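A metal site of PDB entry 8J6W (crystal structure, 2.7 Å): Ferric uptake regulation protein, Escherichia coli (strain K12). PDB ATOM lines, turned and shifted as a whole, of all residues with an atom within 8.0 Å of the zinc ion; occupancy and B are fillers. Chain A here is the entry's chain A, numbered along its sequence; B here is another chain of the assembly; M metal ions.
N of Asp 89 sits at hydrogen-bond distance from O of Phe 102 (2.7 Å).
OE1 of Gln 111 sits close to NE2 of His 125 (3.4 Å).
OD2 of Asp 89 binds the zinc ion, at 1.9 Å.
OE2 of Glu 108 is bound to the zinc ion (2.1 Å).
The zinc ion is bound by a ring nitrogen (NE2) of His 125 (2.2 Å).
The zinc ion is bound by NE2 of His 87 (2.3 Å).
The zinc ion has four donor atoms within binding distance.
Slightly farther from the zinc ion lies OE1 of Glu 108 (2.8 Å).
Slightly farther from the zinc ion lies OD1 of Asp 89 (2.8 Å).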
ATOM      1  N   HIS A  87      -5.888   1.253  29.786  1.00  0.00           N
ATOM      2  CA  HIS A  87      -5.035   0.838  28.673  1.00  0.00           C
ATOM      3  C   HIS A  87      -5.538  -0.460  28.059  1.00  0.00           C
ATOM      4  O   HIS A  87      -5.801  -1.443  28.753  1.00  0.00           O
ATOM      5  CB  HIS A  87      -3.591   0.620  29.097  1.00  0.00           C
ATOM      6  CG  HIS A  87      -2.710   0.204  27.969  1.00  0.00           C
ATOM      7  ND1 HIS A  87      -2.320   1.074  26.972  1.00  0.00           N
ATOM      8  CD2 HIS A  87      -2.177  -1.001  27.641  1.00  0.00           C
ATOM      9  CE1 HIS A  87      -1.561   0.429  26.103  1.00  0.00           C
ATOM     10  NE2 HIS A  87      -1.457  -0.827  26.490  1.00  0.00           N
ATOM     11  N   HIS A  88      -5.628  -0.458  26.739  1.00  0.00           N
ATOM     12  CA  HIS A  88      -5.893  -1.688  26.011  1.00  0.00           C
ATOM     13  C   HIS A  88      -5.097  -1.623  24.713  1.00  0.00           C
ATOM     14  O   HIS A  88      -4.543  -0.593  24.358  1.00  0.00           O
ATOM     15  CB  HIS A  88      -7.386  -1.856  25.752  1.00  0.00           C
ATOM     16  CG  HIS A  88      -7.998  -0.715  25.012  1.00  0.00           C
ATOM     17  ND1 HIS A  88      -8.895   0.151  25.594  1.00  0.00           N
ATOM     18  CD2 HIS A  88      -7.818  -0.274  23.745  1.00  0.00           C
ATOM     19  CE1 HIS A  88      -9.268   1.054  24.703  1.00  0.00           C
ATOM     20  NE2 HIS A  88      -8.627   0.819  23.581  1.00  0.00           N
ATOM     21  N   ASP A  89      -5.052  -2.746  24.022  1.00  0.00           N
ATOM     22  CA  ASP A  89      -4.489  -2.809  22.688  1.00  0.00           C
ATOM     23  C   ASP A  89      -5.628  -3.186  21.745  1.00  0.00           C
ATOM     24  O   ASP A  89      -6.797  -3.191  22.142  1.00  0.00           O
ATOM     25  CB  ASP A  89      -3.298  -3.758  22.668  1.00  0.00           C
ATOM     26  CG  ASP A  89      -2.097  -3.189  23.404  1.00  0.00           C
ATOM     27  OD1 ASP A  89      -1.599  -2.095  23.031  1.00  0.00           O
ATOM     28  OD2 ASP A  89      -1.702  -3.821  24.397  1.00  0.00           O
ATOM     29  N   HIS A  90      -5.307  -3.479  20.495  1.00  0.00           N
ATOM     30  CA  HIS A  90      -6.353  -3.554  19.479  1.00  0.00           C
ATOM     31  C   HIS A  90      -6.244  -4.813  18.644  1.00  0.00           C
ATOM     32  O   HIS A  90      -5.179  -5.096  18.086  1.00  0.00           O
ATOM     33  CB  HIS A  90      -6.329  -2.323  18.580  1.00  0.00           C
ATOM     34  CG  HIS A  90      -6.453  -1.044  19.335  1.00  0.00           C
ATOM     35  ND1 HIS A  90      -5.367  -0.283  19.698  1.00  0.00           N
ATOM     36  CD2 HIS A  90      -7.544  -0.383  19.793  1.00  0.00           C
ATOM     37  CE1 HIS A  90      -5.779   0.787  20.345  1.00  0.00           C
ATOM     38  NE2 HIS A  90      -7.089   0.761  20.404  1.00  0.00           N
ATOM     39  N   PHE A 102      -8.478  -5.225  24.118  1.00  0.00           N
ATOM     40  CA  PHE A 102      -7.972  -6.317  24.936  1.00  0.00           C
ATOM     41  C   PHE A 102      -6.771  -5.828  25.731  1.00  0.00           C
ATOM     42  O   PHE A 102      -6.033  -4.932  25.303  1.00  0.00           O
ATOM     43  CB  PHE A 102      -7.589  -7.566  24.109  1.00  0.00           C
ATOM     44  CG  PHE A 102      -6.284  -7.448  23.317  1.00  0.00           C
ATOM     45  CD1 PHE A 102      -5.054  -7.749  23.885  1.00  0.00           C
ATOM     46  CD2 PHE A 102      -6.314  -7.115  21.970  1.00  0.00           C
ATOM     47  CE1 PHE A 102      -3.875  -7.640  23.161  1.00  0.00           C
ATOM     48  CE2 PHE A 102      -5.140  -7.016  21.225  1.00  0.00           C
ATOM     49  CZ  PHE A 102      -3.922  -7.277  21.827  1.00  0.00           C
ATOM     50  N   SER A 103      -6.585  -6.435  26.899  1.00  0.00           N
ATOM     51  CA  SER A 103      -5.427  -6.154  27.717  1.00  0.00           C
ATOM     52  C   SER A 103      -4.974  -7.460  28.341  1.00  0.00           C
ATOM     53  O   SER A 103      -5.801  -8.239  28.845  1.00  0.00           O
ATOM     54  CB  SER A 103      -5.717  -5.101  28.801  1.00  0.00           C
ATOM     55  OG  SER A 103      -4.576  -4.921  29.626  1.00  0.00           O
ATOM     56  N   ASP A 104      -3.671  -7.713  28.275  1.00  0.00           N
ATOM     57  CA  ASP A 104      -3.046  -8.926  28.781  1.00  0.00           C
ATOM     58  C   ASP A 104      -1.980  -8.473  29.773  1.00  0.00           C
ATOM     59  O   ASP A 104      -1.092  -7.694  29.409  1.00  0.00           O
ATOM     60  CB  ASP A 104      -2.455  -9.749  27.626  1.00  0.00           C
ATOM     61  CG  ASP A 104      -2.193 -11.210  27.993  1.00  0.00           C
ATOM     62  OD1 ASP A 104      -1.391 -11.457  28.932  1.00  0.00           O
ATOM     63  OD2 ASP A 104      -2.761 -12.110  27.325  1.00  0.00           O
ATOM     64  N   ILE A 107       1.555  -9.889  28.957  1.00  0.00           N
ATOM     65  CA  ILE A 107       2.244  -9.234  27.847  1.00  0.00           C
ATOM     66  C   ILE A 107       2.779  -7.870  28.280  1.00  0.00           C
ATOM     67  O   ILE A 107       3.953  -7.576  28.088  1.00  0.00           O
ATOM     68  CB  ILE A 107       1.317  -9.106  26.629  1.00  0.00           C
ATOM     69  CG1 ILE A 107       0.953 -10.485  26.077  1.00  0.00           C
ATOM     70  CG2 ILE A 107       2.001  -8.286  25.531  1.00  0.00           C
ATOM     71  CD1 ILE A 107       0.221 -10.435  24.741  1.00  0.00           C
ATOM     72  N   GLU A 108       1.930  -7.032  28.878  1.00  0.00           N
ATOM     73  CA  GLU A 108       2.386  -5.721  29.324  1.00  0.00           C
ATOM     74  C   GLU A 108       3.582  -5.854  30.266  1.00  0.00           C
ATOM     75  O   GLU A 108       4.406  -4.940  30.356  1.00  0.00           O
ATOM     76  CB  GLU A 108       1.269  -4.928  30.032  1.00  0.00           C
ATOM     77  CG  GLU A 108      -0.051  -4.827  29.260  1.00  0.00           C
ATOM     78  CD  GLU A 108      -0.018  -3.903  28.030  1.00  0.00           C
ATOM     79  OE1 GLU A 108       0.604  -2.816  28.070  1.00  0.00           O
ATOM     80  OE2 GLU A 108      -0.647  -4.250  27.014  1.00  0.00           O
ATOM     81  N   GLN A 111       6.711  -6.964  28.066  1.00  0.00           N
ATOM     82  CA  GLN A 111       7.125  -5.788  27.311  1.00  0.00           C
ATOM     83  C   GLN A 111       8.032  -4.908  28.157  1.00  0.00           C
ATOM     84  O   GLN A 111       9.070  -4.426  27.684  1.00  0.00           O
ATOM     85  CB  GLN A 111       5.914  -5.020  26.836  1.00  0.00           C
ATOM     86  CG  GLN A 111       5.196  -5.651  25.662  1.00  0.00           C
ATOM     87  CD  GLN A 111       3.916  -4.911  25.280  1.00  0.00           C
ATOM     88  OE1 GLN A 111       3.503  -3.968  25.958  1.00  0.00           O
ATOM     89  NE2 GLN A 111       3.274  -5.356  24.213  1.00  0.00           N
ATOM     90  N   LEU A 122      10.452   1.205  29.443  1.00  0.00           N
ATOM     91  CA  LEU A 122       9.315   1.297  28.545  1.00  0.00           C
ATOM     92  C   LEU A 122       8.403   2.440  28.915  1.00  0.00           C
ATOM     93  O   LEU A 122       7.872   2.480  30.033  1.00  0.00           O
ATOM     94  CB  LEU A 122       8.525  -0.017  28.583  1.00  0.00           C
ATOM     95  CG  LEU A 122       7.439  -0.113  27.518  1.00  0.00           C
ATOM     96  CD1 LEU A 122       8.082  -0.281  26.104  1.00  0.00           C
ATOM     97  CD2 LEU A 122       6.593  -1.290  27.857  1.00  0.00           C
ATOM     98  N   ASN A 124       6.074   3.909  26.133  1.00  0.00           N
ATOM     99  CA  ASN A 124       4.881   3.804  25.311  1.00  0.00           C
ATOM    100  C   ASN A 124       5.026   2.598  24.392  1.00  0.00           C
ATOM    101  O   ASN A 124       6.130   2.066  24.208  1.00  0.00           O
ATOM    102  CB  ASN A 124       4.652   5.091  24.513  1.00  0.00           C
ATOM    103  CG  ASN A 124       3.300   5.126  23.820  1.00  0.00           C
ATOM    104  OD1 ASN A 124       2.336   4.516  24.282  1.00  0.00           O
ATOM    105  ND2 ASN A 124       3.217   5.861  22.724  1.00  0.00           N
ATOM    106  N   HIS A 125       3.900   2.168  23.839  1.00  0.00           N
ATOM    107  CA  HIS A 125       3.890   1.016  22.956  1.00  0.00           C
ATOM    108  C   HIS A 125       2.577   0.987  22.210  1.00  0.00           C
ATOM    109  O   HIS A 125       1.572   1.528  22.674  1.00  0.00           O
ATOM    110  CB  HIS A 125       4.104  -0.289  23.724  1.00  0.00           C
ATOM    111  CG  HIS A 125       2.986  -0.653  24.636  1.00  0.00           C
ATOM    112  ND1 HIS A 125       2.845  -0.117  25.897  1.00  0.00           N
ATOM    113  CD2 HIS A 125       1.945  -1.509  24.478  1.00  0.00           C
ATOM    114  CE1 HIS A 125       1.763  -0.614  26.473  1.00  0.00           C
ATOM    115  NE2 HIS A 125       1.204  -1.458  25.634  1.00  0.00           N
ATOM    116  N   SER A 126       2.593   0.358  21.042  1.00  0.00           N
ATOM    117  CA  SER A 126       1.369   0.090  20.310  1.00  0.00           C
ATOM    118  C   SER A 126       1.411  -1.327  19.791  1.00  0.00           C
ATOM    119  O   SER A 126       2.425  -1.784  19.240  1.00  0.00           O
ATOM    120  CB  SER A 126       1.137   1.097  19.181  1.00  0.00           C
ATOM    121  OG  SER A 126       1.964   0.856  18.081  1.00  0.00           O
ATOM    122  N   LEU A 127       0.302  -2.035  19.988  1.00  0.00           N
ATOM    123  CA  LEU A 127       0.202  -3.427  19.609  1.00  0.00           C
ATOM    124  C   LEU A 127      -1.074  -3.573  18.806  1.00  0.00           C
ATOM    125  O   LEU A 127      -2.159  -3.424  19.347  1.00  0.00           O
ATOM    126  CB  LEU A 127       0.213  -4.336  20.839  1.00  0.00           C
ATOM    127  CG  LEU A 127      -0.145  -5.809  20.674  1.00  0.00           C
ATOM    128  CD1 LEU A 127       0.641  -6.488  19.567  1.00  0.00           C
ATOM    129  CD2 LEU A 127       0.135  -6.458  22.005  1.00  0.00           C
ATOM    130  N   LEU B 127       4.069  -4.794  16.565  1.00  0.00           N
ATOM    131  CA  LEU B 127       4.292  -4.496  17.962  1.00  0.00           C
ATOM    132  C   LEU B 127       5.478  -3.556  18.026  1.00  0.00           C
ATOM    133  O   LEU B 127       6.592  -3.952  17.715  1.00  0.00           O
ATOM    134  CB  LEU B 127       4.529  -5.774  18.767  1.00  0.00           C
ATOM    135  CG  LEU B 127       5.041  -5.663  20.199  1.00  0.00           C
ATOM    136  CD1 LEU B 127       4.224  -4.705  21.047  1.00  0.00           C
ATOM    137  CD2 LEU B 127       4.994  -7.057  20.769  1.00  0.00           C
ATOM    138  N   LEU B 129       7.648  -1.058  20.530  1.00  0.00           N
ATOM    139  CA  LEU B 129       7.946  -0.653  21.886  1.00  0.00           C
ATOM    140  C   LEU B 129       8.780   0.612  21.853  1.00  0.00           C
ATOM    141  O   LEU B 129       9.707   0.738  21.053  1.00  0.00           O
ATOM    142  CB  LEU B 129       8.698  -1.750  22.658  1.00  0.00           C
ATOM    143  CG  LEU B 129       7.977  -3.084  22.885  1.00  0.00           C
ATOM    144  CD1 LEU B 129       8.781  -4.006  23.775  1.00  0.00           C
ATOM    145  CD2 LEU B 129       6.575  -2.861  23.451  1.00  0.00           C
HETATM  146 ZN    ZN M   1      -0.621  -2.747  25.607  1.00  0.00          ZN
